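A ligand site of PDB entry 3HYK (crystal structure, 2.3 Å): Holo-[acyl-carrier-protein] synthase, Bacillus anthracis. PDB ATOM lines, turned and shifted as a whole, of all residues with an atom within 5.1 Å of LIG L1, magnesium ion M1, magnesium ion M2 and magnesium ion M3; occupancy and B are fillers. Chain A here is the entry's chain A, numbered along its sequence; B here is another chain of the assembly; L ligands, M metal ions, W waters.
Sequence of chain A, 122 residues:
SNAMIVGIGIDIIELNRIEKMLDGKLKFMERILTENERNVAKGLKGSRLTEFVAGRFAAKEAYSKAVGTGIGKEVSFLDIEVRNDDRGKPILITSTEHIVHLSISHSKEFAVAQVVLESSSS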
ATOM      1  N   ARG A  48     -24.684  30.597 -15.954  1.00  0.00           N
ATOM      2  CA  ARG A  48     -25.455  29.398 -16.125  1.00  0.00           C
ATOM      3  C   ARG A  48     -26.959  29.694 -16.072  1.00  0.00           C
ATOM      4  O   ARG A  48     -27.732  29.196 -16.895  1.00  0.00           O
ATOM      5  CB  ARG A  48     -25.010  28.344 -15.098  1.00  0.00           C
ATOM      6  CG  ARG A  48     -25.761  27.037 -15.172  1.00  0.00           C
ATOM      7  CD  ARG A  48     -25.883  26.544 -16.617  1.00  0.00           C
ATOM      8  NE  ARG A  48     -26.827  25.428 -16.689  1.00  0.00           N
ATOM      9  CZ  ARG A  48     -27.403  24.988 -17.795  1.00  0.00           C
ATOM     10  NH1 ARG A  48     -27.186  25.571 -18.964  1.00  0.00           N
ATOM     11  NH2 ARG A  48     -28.254  23.971 -17.706  1.00  0.00           N
ATOM     12  N   GLU A  51     -27.827  31.656 -19.373  1.00  0.00           N
ATOM     13  CA  GLU A  51     -27.887  30.813 -20.564  1.00  0.00           C
ATOM     14  C   GLU A  51     -29.093  29.866 -20.467  1.00  0.00           C
ATOM     15  O   GLU A  51     -29.763  29.614 -21.457  1.00  0.00           O
ATOM     16  CB  GLU A  51     -26.567  30.047 -20.797  1.00  0.00           C
ATOM     17  CG  GLU A  51     -26.284  28.914 -19.829  1.00  0.00           C
ATOM     18  CD  GLU A  51     -24.941  28.225 -20.067  1.00  0.00           C
ATOM     19  OE1 GLU A  51     -24.095  28.806 -20.771  1.00  0.00           O
ATOM     20  OE2 GLU A  51     -24.731  27.109 -19.531  1.00  0.00           O
ATOM     21  N   PHE A  52     -29.394  29.396 -19.266  1.00  0.00           N
ATOM     22  CA  PHE A  52     -30.530  28.489 -19.075  1.00  0.00           C
ATOM     23  C   PHE A  52     -31.859  29.159 -19.424  1.00  0.00           C
ATOM     24  O   PHE A  52     -32.698  28.581 -20.133  1.00  0.00           O
ATOM     25  CB  PHE A  52     -30.561  27.995 -17.635  1.00  0.00           C
ATOM     26  CG  PHE A  52     -31.720  27.112 -17.338  1.00  0.00           C
ATOM     27  CD1 PHE A  52     -31.695  25.774 -17.677  1.00  0.00           C
ATOM     28  CD2 PHE A  52     -32.832  27.603 -16.699  1.00  0.00           C
ATOM     29  CE1 PHE A  52     -32.758  24.948 -17.402  1.00  0.00           C
ATOM     30  CE2 PHE A  52     -33.900  26.769 -16.428  1.00  0.00           C
ATOM     31  CZ  PHE A  52     -33.857  25.444 -16.766  1.00  0.00           C
ATOM     32  N   ARG A  56     -34.315  28.385 -22.783  1.00  0.00           N
ATOM     33  CA  ARG A  56     -35.719  28.098 -22.638  1.00  0.00           C
ATOM     34  C   ARG A  56     -36.555  29.044 -23.457  1.00  0.00           C
ATOM     35  O   ARG A  56     -37.503  28.616 -24.147  1.00  0.00           O
ATOM     36  CB  ARG A  56     -36.151  28.133 -21.174  1.00  0.00           C
ATOM     37  CG  ARG A  56     -36.142  26.780 -20.508  1.00  0.00           C
ATOM     38  CD  ARG A  56     -34.878  25.985 -20.762  1.00  0.00           C
ATOM     39  NE  ARG A  56     -34.984  24.635 -20.213  1.00  0.00           N
ATOM     40  CZ  ARG A  56     -34.067  23.688 -20.379  1.00  0.00           C
ATOM     41  NH1 ARG A  56     -32.985  23.945 -21.095  1.00  0.00           N
ATOM     42  NH2 ARG A  56     -34.246  22.488 -19.846  1.00  0.00           N
ATOM     43  N   ASN A  84     -34.614  18.501 -19.327  1.00  0.00           N
ATOM     44  CA  ASN A  84     -33.499  17.737 -19.856  1.00  0.00           C
ATOM     45  C   ASN A  84     -33.640  16.289 -19.385  1.00  0.00           C
ATOM     46  O   ASN A  84     -34.065  16.053 -18.244  1.00  0.00           O
ATOM     47  CB  ASN A  84     -32.199  18.319 -19.326  1.00  0.00           C
ATOM     48  CG  ASN A  84     -31.996  19.757 -19.785  1.00  0.00           C
ATOM     49  OD1 ASN A  84     -32.374  20.680 -19.076  1.00  0.00           O
ATOM     50  ND2 ASN A  84     -31.489  19.946 -20.986  1.00  0.00           N
ATOM     51  N   ARG A  87     -29.516  12.229 -19.973  1.00  0.00           N
ATOM     52  CA  ARG A  87     -28.287  12.432 -20.721  1.00  0.00           C
ATOM     53  C   ARG A  87     -28.061  13.927 -20.957  1.00  0.00           C
ATOM     54  O   ARG A  87     -27.031  14.327 -21.491  1.00  0.00           O
ATOM     55  CB  ARG A  87     -28.339  11.697 -22.054  1.00  0.00           C
ATOM     56  CG  ARG A  87     -28.545  10.160 -21.967  1.00  0.00           C
ATOM     57  CD  ARG A  87     -27.439   9.483 -21.134  1.00  0.00           C
ATOM     58  NE  ARG A  87     -26.100   9.743 -21.653  1.00  0.00           N
ATOM     59  CZ  ARG A  87     -25.378   8.921 -22.419  1.00  0.00           C
ATOM     60  NH1 ARG A  87     -25.833   7.733 -22.781  1.00  0.00           N
ATOM     61  NH2 ARG A  87     -24.168   9.287 -22.814  1.00  0.00           N
ATOM     62  N   GLY A  88     -29.037  14.751 -20.559  1.00  0.00           N
ATOM     63  CA  GLY A  88     -28.971  16.201 -20.724  1.00  0.00           C
ATOM     64  C   GLY A  88     -29.720  16.693 -21.939  1.00  0.00           C
ATOM     65  O   GLY A  88     -29.776  17.904 -22.196  1.00  0.00           O
ATOM     66  N   LYS A  89     -30.294  15.768 -22.712  1.00  0.00           N
ATOM     67  CA  LYS A  89     -31.035  16.154 -23.908  1.00  0.00           C
ATOM     68  C   LYS A  89     -32.312  16.902 -23.556  1.00  0.00           C
ATOM     69  O   LYS A  89     -33.110  16.416 -22.756  1.00  0.00           O
ATOM     70  CB  LYS A  89     -31.382  14.935 -24.777  1.00  0.00           C
ATOM     71  CG  LYS A  89     -32.339  15.270 -25.947  1.00  0.00           C
ATOM     72  CD  LYS A  89     -32.419  14.140 -26.954  1.00  0.00           C
ATOM     73  CE  LYS A  89     -32.950  12.827 -26.355  1.00  0.00           C
ATOM     74  NZ  LYS A  89     -32.726  11.626 -27.254  1.00  0.00           N
ATOM     75  N   PRO A  90     -32.510  18.102 -24.157  1.00  0.00           N
ATOM     76  CA  PRO A  90     -33.719  18.912 -23.908  1.00  0.00           C
ATOM     77  C   PRO A  90     -34.986  18.299 -24.512  1.00  0.00           C
ATOM     78  O   PRO A  90     -35.009  17.990 -25.699  1.00  0.00           O
ATOM     79  CB  PRO A  90     -33.409  20.216 -24.630  1.00  0.00           C
ATOM     80  CG  PRO A  90     -32.462  19.842 -25.721  1.00  0.00           C
ATOM     81  CD  PRO A  90     -31.607  18.754 -25.122  1.00  0.00           C
ATOM     82  N   ILE A 104     -30.768  22.803 -28.428  1.00  0.00           N
ATOM     83  CA  ILE A 104     -30.335  24.092 -27.896  1.00  0.00           C
ATOM     84  C   ILE A 104     -28.802  24.136 -27.876  1.00  0.00           C
ATOM     85  O   ILE A 104     -28.145  23.105 -27.804  1.00  0.00           O
ATOM     86  CB  ILE A 104     -30.809  24.249 -26.432  1.00  0.00           C
ATOM     87  CG1 ILE A 104     -32.341  24.248 -26.342  1.00  0.00           C
ATOM     88  CG2 ILE A 104     -30.227  25.518 -25.801  1.00  0.00           C
ATOM     89  CD1 ILE A 104     -32.892  24.025 -24.928  1.00  0.00           C
ATOM     90  N   SER A 105     -28.261  25.340 -27.969  1.00  0.00           N
ATOM     91  CA  SER A 105     -26.826  25.546 -27.827  1.00  0.00           C
ATOM     92  C   SER A 105     -26.621  26.975 -27.357  1.00  0.00           C
ATOM     93  O   SER A 105     -27.370  27.876 -27.732  1.00  0.00           O
ATOM     94  CB  SER A 105     -26.067  25.330 -29.147  1.00  0.00           C
ATOM     95  OG  SER A 105     -24.664  25.566 -28.960  1.00  0.00           O
ATOM     96  N   HIS A 106     -25.608  27.167 -26.533  1.00  0.00           N
ATOM     97  CA  HIS A 106     -25.282  28.499 -26.044  1.00  0.00           C
ATOM     98  C   HIS A 106     -23.784  28.741 -25.878  1.00  0.00           C
ATOM     99  O   HIS A 106     -23.095  28.030 -25.176  1.00  0.00           O
ATOM    100  CB  HIS A 106     -26.054  28.837 -24.741  1.00  0.00           C
ATOM    101  CG  HIS A 106     -26.319  27.663 -23.847  1.00  0.00           C
ATOM    102  ND1 HIS A 106     -25.315  26.916 -23.259  1.00  0.00           N
ATOM    103  CD2 HIS A 106     -27.489  27.167 -23.371  1.00  0.00           C
ATOM    104  CE1 HIS A 106     -25.867  25.976 -22.517  1.00  0.00           C
ATOM    105  NE2 HIS A 106     -27.177  26.098 -22.567  1.00  0.00           N
ATOM    106  N   SER A 107     -23.272  29.738 -26.593  1.00  0.00           N
ATOM    107  CA  SER A 107     -21.884  30.105 -26.443  1.00  0.00           C
ATOM    108  C   SER A 107     -21.864  31.116 -25.301  1.00  0.00           C
ATOM    109  O   SER A 107     -22.829  31.255 -24.545  1.00  0.00           O
ATOM    110  CB  SER A 107     -21.309  30.723 -27.720  1.00  0.00           C
ATOM    111  OG  SER A 107     -21.904  31.966 -28.023  1.00  0.00           O
ATOM    112  N   ILE B  10     -28.066  21.111 -32.871  1.00  0.00           N
ATOM    113  CA  ILE B  10     -27.549  22.387 -33.363  1.00  0.00           C
ATOM    114  C   ILE B  10     -26.393  22.811 -32.467  1.00  0.00           C
ATOM    115  O   ILE B  10     -26.338  22.463 -31.299  1.00  0.00           O
ATOM    116  CB  ILE B  10     -28.653  23.496 -33.410  1.00  0.00           C
ATOM    117  CG1 ILE B  10     -28.195  24.683 -34.261  1.00  0.00           C
ATOM    118  CG2 ILE B  10     -29.037  23.948 -31.991  1.00  0.00           C
ATOM    119  CD1 ILE B  10     -29.290  25.689 -34.632  1.00  0.00           C
ATOM    120  N   ASP B  11     -25.452  23.565 -33.007  1.00  0.00           N
ATOM    121  CA  ASP B  11     -24.362  24.038 -32.174  1.00  0.00           C
ATOM    122  C   ASP B  11     -23.872  25.370 -32.718  1.00  0.00           C
ATOM    123  O   ASP B  11     -23.854  25.565 -33.930  1.00  0.00           O
ATOM    124  CB  ASP B  11     -23.201  23.036 -32.199  1.00  0.00           C
ATOM    125  CG  ASP B  11     -22.153  23.315 -31.119  1.00  0.00           C
ATOM    126  OD1 ASP B  11     -22.560  23.741 -29.997  1.00  0.00           O
ATOM    127  OD2 ASP B  11     -20.945  23.071 -31.371  1.00  0.00           O
ATOM    128  N   ILE B  12     -23.503  26.266 -31.807  1.00  0.00           N
ATOM    129  CA  ILE B  12     -22.942  27.563 -32.178  1.00  0.00           C
ATOM    130  C   ILE B  12     -21.616  27.683 -31.440  1.00  0.00           C
ATOM    131  O   ILE B  12     -21.553  27.418 -30.234  1.00  0.00           O
ATOM    132  CB  ILE B  12     -23.896  28.765 -31.873  1.00  0.00           C
ATOM    133  CG1 ILE B  12     -23.261  30.082 -32.356  1.00  0.00           C
ATOM    134  CG2 ILE B  12     -24.254  28.841 -30.387  1.00  0.00           C
ATOM    135  CD1 ILE B  12     -24.220  31.289 -32.418  1.00  0.00           C
ATOM    136  N   ILE B  13     -20.554  28.031 -32.152  1.00  0.00           N
ATOM    137  CA  ILE B  13     -19.223  28.161 -31.567  1.00  0.00           C
ATOM    138  C   ILE B  13     -18.575  29.505 -31.891  1.00  0.00           C
ATOM    139  O   ILE B  13     -18.584  29.965 -33.034  1.00  0.00           O
ATOM    140  CB  ILE B  13     -18.243  27.074 -32.092  1.00  0.00           C
ATOM    141  CG1 ILE B  13     -18.726  25.681 -31.719  1.00  0.00           C
ATOM    142  CG2 ILE B  13     -16.830  27.290 -31.510  1.00  0.00           C
ATOM    143  CD1 ILE B  13     -17.835  24.566 -32.302  1.00  0.00           C
ATOM    144  N   GLU B  61     -20.438  17.824 -32.833  1.00  0.00           N
ATOM    145  CA  GLU B  61     -21.209  18.029 -31.616  1.00  0.00           C
ATOM    146  C   GLU B  61     -22.701  18.032 -31.905  1.00  0.00           C
ATOM    147  O   GLU B  61     -23.508  17.435 -31.195  1.00  0.00           O
ATOM    148  CB  GLU B  61     -20.788  19.347 -30.920  1.00  0.00           C
ATOM    149  CG  GLU B  61     -21.526  19.598 -29.654  1.00  0.00           C
ATOM    150  CD  GLU B  61     -21.009  20.792 -28.863  1.00  0.00           C
ATOM    151  OE1 GLU B  61     -19.788  21.010 -28.843  1.00  0.00           O
ATOM    152  OE2 GLU B  61     -21.832  21.480 -28.223  1.00  0.00           O
ATOM    153  N   SER B  64     -23.864  14.636 -32.331  1.00  0.00           N
ATOM    154  CA  SER B  64     -23.896  13.905 -31.065  1.00  0.00           C
ATOM    155  C   SER B  64     -25.130  14.303 -30.247  1.00  0.00           C
ATOM    156  O   SER B  64     -25.600  13.549 -29.406  1.00  0.00           O
ATOM    157  CB  SER B  64     -22.602  14.140 -30.267  1.00  0.00           C
ATOM    158  OG  SER B  64     -22.504  15.486 -29.792  1.00  0.00           O
ATOM    159  N   LYS B  65     -25.627  15.505 -30.469  1.00  0.00           N
ATOM    160  CA  LYS B  65     -26.833  15.943 -29.790  1.00  0.00           C
ATOM    161  C   LYS B  65     -28.029  15.300 -30.505  1.00  0.00           C
ATOM    162  O   LYS B  65     -29.023  14.942 -29.883  1.00  0.00           O
ATOM    163  CB  LYS B  65     -26.964  17.470 -29.803  1.00  0.00           C
ATOM    164  CG  LYS B  65     -25.958  18.259 -28.955  1.00  0.00           C
ATOM    165  CD  LYS B  65     -26.314  19.789 -29.021  1.00  0.00           C
ATOM    166  CE  LYS B  65     -25.281  20.682 -28.371  1.00  0.00           C
ATOM    167  NZ  LYS B  65     -25.591  22.154 -28.471  1.00  0.00           N
ATOM    168  N   GLY B  68     -28.615  12.138 -29.166  1.00  0.00           N
ATOM    169  CA  GLY B  68     -29.140  12.268 -27.796  1.00  0.00           C
ATOM    170  C   GLY B  68     -28.142  12.008 -26.687  1.00  0.00           C
ATOM    171  O   GLY B  68     -28.463  12.068 -25.497  1.00  0.00           O
ATOM    172  N   THR B  69     -26.903  11.752 -27.055  1.00  0.00           N
ATOM    173  CA  THR B  69     -25.898  11.437 -26.041  1.00  0.00           C
ATOM    174  C   THR B  69     -24.823  12.512 -25.822  1.00  0.00           C
ATOM    175  O   THR B  69     -24.225  12.577 -24.762  1.00  0.00           O
ATOM    176  CB  THR B  69     -25.187  10.139 -26.444  1.00  0.00           C
ATOM    177  OG1 THR B  69     -24.557  10.334 -27.713  1.00  0.00           O
ATOM    178  CG2 THR B  69     -26.211   8.983 -26.560  1.00  0.00           C
ATOM    179  N   GLY B  70     -24.581  13.353 -26.814  1.00  0.00           N
ATOM    180  CA  GLY B  70     -23.477  14.317 -26.751  1.00  0.00           C
ATOM    181  C   GLY B  70     -22.178  13.535 -26.970  1.00  0.00           C
ATOM    182  O   GLY B  70     -22.213  12.296 -27.103  1.00  0.00           O
HETATM  183  P1  LIG L   1     -29.240  23.413 -21.309  1.00  0.00           P
HETATM  184  O1  LIG L   1     -29.361  24.899 -21.060  1.00  0.00           O
HETATM  185  O2  LIG L   1     -28.293  22.729 -20.403  1.00  0.00           O
HETATM  186  O3  LIG L   1     -30.543  22.691 -21.567  1.00  0.00           O
HETATM  187  P2  LIG L   1     -23.820  23.712 -25.869  1.00  0.00           P
HETATM  188  O4  LIG L   1     -22.999  22.948 -24.872  1.00  0.00           O
HETATM  189  O5  LIG L   1     -23.937  25.126 -25.368  1.00  0.00           O
HETATM  190  O6  LIG L   1     -23.506  23.589 -27.355  1.00  0.00           O
HETATM  191  O7  LIG L   1     -25.306  23.145 -25.787  1.00  0.00           O
HETATM  192  C1  LIG L   1     -25.945  23.246 -24.520  1.00  0.00           C
HETATM  193  C2  LIG L   1     -27.222  22.452 -24.596  1.00  0.00           C
HETATM  194  O8  LIG L   1     -26.970  21.158 -25.145  1.00  0.00           O
HETATM  195  C3  LIG L   1     -27.880  22.187 -23.270  1.00  0.00           C
HETATM  196  O9  LIG L   1     -28.489  23.358 -22.747  1.00  0.00           O
HETATM  197  C4  LIG L   1     -28.795  21.009 -23.642  1.00  0.00           C
HETATM  198  O10 LIG L   1     -30.126  21.392 -23.990  1.00  0.00           O
HETATM  199  C5  LIG L   1     -28.102  20.369 -24.840  1.00  0.00           C
HETATM  200  N1  LIG L   1     -27.677  19.010 -24.466  1.00  0.00           N
HETATM  201  C6  LIG L   1     -27.019  18.650 -23.344  1.00  0.00           C
HETATM  202  N2  LIG L   1     -26.818  17.312 -23.310  1.00  0.00           N
HETATM  203  C7  LIG L   1     -27.378  16.810 -24.421  1.00  0.00           C
HETATM  204  C8  LIG L   1     -27.538  15.459 -24.994  1.00  0.00           C
HETATM  205  N3  LIG L   1     -27.038  14.372 -24.345  1.00  0.00           N
HETATM  206  N4  LIG L   1     -28.197  15.375 -26.178  1.00  0.00           N
HETATM  207  C9  LIG L   1     -28.698  16.449 -26.824  1.00  0.00           C
HETATM  208  N5  LIG L   1     -28.591  17.712 -26.353  1.00  0.00           N
HETATM  209  C10 LIG L   1     -27.937  17.929 -25.196  1.00  0.00           C
HETATM  210  P1  LG2 L   2     -19.926  22.862 -22.711  1.00  0.00           P
HETATM  211  O1  LG2 L   2     -19.844  24.338 -22.993  1.00  0.00           O
HETATM  212  O2  LG2 L   2     -20.589  22.566 -21.394  1.00  0.00           O
HETATM  213  O3  LG2 L   2     -20.432  22.096 -23.906  1.00  0.00           O
HETATM  214  P2  LG2 L   2     -15.719  24.867 -18.113  1.00  0.00           P
HETATM  215  O4  LG2 L   2     -16.270  23.652 -17.403  1.00  0.00           O
HETATM  216  O5  LG2 L   2     -16.072  26.187 -17.453  1.00  0.00           O
HETATM  217  O6  LG2 L   2     -14.273  24.777 -18.546  1.00  0.00           O
HETATM  218  O7  LG2 L   2     -16.556  24.862 -19.514  1.00  0.00           O
HETATM  219  C1  LG2 L   2     -15.867  24.618 -20.746  1.00  0.00           C
HETATM  220  C2  LG2 L   2     -16.681  23.988 -21.860  1.00  0.00           C
HETATM  221  O8  LG2 L   2     -15.682  23.633 -22.807  1.00  0.00           O
HETATM  222  C3  LG2 L   2     -17.428  22.677 -21.537  1.00  0.00           C
HETATM  223  O9  LG2 L   2     -18.388  22.318 -22.549  1.00  0.00           O
HETATM  224  C4  LG2 L   2     -16.260  21.720 -21.556  1.00  0.00           C
HETATM  225  O10 LG2 L   2     -16.625  20.354 -21.748  1.00  0.00           O
HETATM  226  C5  LG2 L   2     -15.474  22.222 -22.768  1.00  0.00           C
HETATM  227  N1  LG2 L   2     -14.042  21.900 -22.672  1.00  0.00           N
HETATM  228  C6  LG2 L   2     -13.241  21.978 -21.590  1.00  0.00           C
HETATM  229  N2  LG2 L   2     -11.981  21.575 -21.924  1.00  0.00           N
HETATM  230  C7  LG2 L   2     -11.984  21.239 -23.233  1.00  0.00           C
HETATM  231  C8  LG2 L   2     -11.013  20.713 -24.223  1.00  0.00           C
HETATM  232  N3  LG2 L   2      -9.728  20.482 -23.877  1.00  0.00           N
HETATM  233  N4  LG2 L   2     -11.435  20.492 -25.490  1.00  0.00           N
HETATM  234  C9  LG2 L   2     -12.711  20.711 -25.852  1.00  0.00           C
HETATM  235  N5  LG2 L   2     -13.637  21.158 -25.000  1.00  0.00           N
HETATM  236  C10 LG2 L   2     -13.346  21.441 -23.718  1.00  0.00           C
HETATM  237 MG    MG M   1     -23.210  26.345 -23.958  1.00  0.00          MG
HETATM  238 MG    MG M   2     -22.257  21.416 -24.024  1.00  0.00          MG
HETATM  239 MG    MG M   3     -21.442  23.650 -28.208  1.00  0.00          MG
HETATM  240  O   HOH W   1     -22.575  27.484 -22.418  1.00  0.00           O
HETATM  241  O   HOH W   2     -22.952  21.949 -22.239  1.00  0.00           O
HETATM  242  O   HOH W   3     -24.141  17.802 -25.308  1.00  0.00           O
HETATM  243  O   HOH W   4     -21.988  20.393 -25.865  1.00  0.00           O
HETATM  244  O   HOH W   5     -24.046  20.265 -24.322  1.00  0.00           O
HETATM  245  O   HOH W   6     -21.789  19.527 -23.221  1.00  0.00           O
HETATM  246  O   HOH W   7     -19.532  23.488 -29.134  1.00  0.00           O
HETATM  247  O   HOH W   8     -24.861  20.299 -21.150  1.00  0.00           O
HETATM  248  O   HOH W   9     -25.834  22.495 -20.084  1.00  0.00           O
HETATM  249  O   HOH W  10     -31.413  26.512 -21.864  1.00  0.00           O
HETATM  250  O   HOH W  11     -21.287  25.820 -24.367  1.00  0.00           O
HETATM  251  O   HOH W  12     -20.778  23.575 -26.269  1.00  0.00           O
HETATM  252  O   HOH W  13     -29.890  19.238 -28.191  1.00  0.00           O
HETATM  253  O   HOH W  14     -27.961  20.005 -20.350  1.00  0.00           O
HETATM  254  O   HOH W  15     -21.629  25.662 -27.975  1.00  0.00           O
HETATM  255  O   HOH W  16     -23.226  24.796 -22.494  1.00  0.00           O
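The backbone NH (N) of His 106 sits close to an oxygen (O5) of LIG L1, at 2.9 Å.
The side-chain amino group (NZ) of Lys 65 of chain B is in hydrogen-bond range of an oxygen (O7) of LIG L1.
The guanidinium group (NH1) of Arg 56 is in salt-bridge range of an oxygen (O3) of LIG L1, 2.8 Å away.
The side-chain hydroxyl of Ser 105 lies close to an oxygen (O6) of LIG L1 (2.8 Å).
O of Arg 87 is in hydrogen-bond range of N3 of LIG L1 (2.9 Å).
O of Gly 68 of chain B is in hydrogen-bond range of N3 of LIG L1.
An oxygen (O3) of LIG L1 sits at hydrogen-bond distance from the side-chain amide nitrogen (ND2) of Asn 84.
The guanidinium group (NH2) of Arg 48 lies within salt-bridge range of an oxygen (O2) of LIG L1 (3.0 Å).
N3 of LIG L1 sits close to O of Thr 69 of chain B (3.4 Å).
The side-chain carboxylate (OD1) of Asp 11 of chain B sits close to the side-chain amino group (NZ) of Lys 65 of chain B (3.7 Å).
The side-chain carboxylate (OD1) of Asp 11 of chain B sits close to the side-chain hydroxyl (OG) of Ser 105, at 3.0 Å.
The backbone carbonyl oxygen (O) of Glu 61 of chain B lies within hydrogen-bond range of the side-chain hydroxyl (OG) of Ser 64 of chain B (2.6 Å).
NZ of Lys 65 of chain B is in hydrogen-bond range of O of Ile 10 of chain B, at 2.9 Å.
N of Ile 12 of chain B lies within hydrogen-bond range of OG of Ser 105.
ND2 of Asn 84 sits at hydrogen-bond distance from O of Gly 88.
NH1 of Arg 48 is in salt-bridge range of OE2 of Glu 51 (3.0 Å).
O of Ser 64 of chain B sits at hydrogen-bond distance from N of Thr 69 of chain B (3.2 Å).
N2 of LIG L1 sits close to O of Gly 88 (3.2 Å).
O of Ile 104 lies close to O7 of LIG L1 (3.5 Å).
Lys 89 touches LIG L1 (CB to N4, 3.5 Å).
Pro 90 touches LIG L1.
Gly 70 of chain B touches LIG L1 (N to N3, 3.6 Å).
16 residues have an atom within 4 Å of LIG L1: Arg 48, Arg 56, Asn 84, Arg 87, Gly 88, Lys 89, Pro 90, Ile 104, Ser 105, His 106, Asp 11 of chain B, Glu 61 of chain B, Lys 65 of chain B, Gly 68 of chain B, Thr 69 of chain B and Gly 70 of chain B.
Of the 23 residues printed, 1 comes within 4 Å of magnesium ion M1.
No residue comes within 4 Å of magnesium ion M2.
The nearest printed residue that does not touch magnesium ion M2 is Glu 61 of chain B (4.2 Å).
Residues that only touch magnesium ion M3: Ser 105.
Within 4 Å of magnesium ion M3: Ser 105, Asp 11 of chain B and Glu 61 of chain B.
O5 of LIG L1 is bound to magnesium ion M1 (2.0 Å).
Water W1 binds magnesium ion M1 (2.0 Å).
Water W11 is bound to magnesium ion M1 (2.0 Å).
The backbone carbonyl oxygen (O) of His 106 is bound to magnesium ion M1 (2.1 Å).
Magnesium ion M1 is bound by water W16 (2.1 Å).
Magnesium ion M1 is bound by a ring nitrogen (ND1) of His 106.
Magnesium ion M1 has six donor atoms within binding distance.
An oxygen (O4) of LIG L1 binds magnesium ion M2.
Magnesium ion M2 is bound by O3 of LG2 L2 (2.0 Å).
Water W2 is bound to magnesium ion M2 (2.0 Å).
Water W6 binds magnesium ion M2.
Water W4 is bound to magnesium ion M2 (2.1 Å).
Magnesium ion M2 is bound by water W5 (2.1 Å).
Magnesium ion M3 is bound by water W15.
Magnesium ion M3 is bound by water W12, 2.1 Å away.
OD1 of Asp 11 of chain B binds magnesium ion M3 (2.1 Å).
Water W7 is bound to magnesium ion M3.
The side-chain carboxylate (OE2) of Glu 61 of chain B is bound to magnesium ion M3 (2.2 Å).
O6 of LIG L1 binds magnesium ion M3 (2.2 Å).
Magnesium ion M3 has six donor atoms within binding distance.
Water W15 lies within hydrogen-bond range of O of Ile 12 of chain B (2.9 Å) and OG of Ser 105 (3.2 Å).
Water W7 bridges the side-chain carboxylate of Glu 61 of chain B (2.5 Å) and the side-chain carboxylate of Asp 11 of chain B (2.7 Å).
Water W10 lies within hydrogen-bond range of an oxygen (O1) of LIG L1 (2.7 Å), the backbone carbonyl oxygen of Phe 52 (3.0 Å) and the guanidinium group of Arg 56 (3.1 Å).
Water W14 lies within hydrogen-bond range of an oxygen (O2) of LIG L1 (2.7 Å) and the backbone carbonyl oxygen (O) of Gly 88 (3.3 Å).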
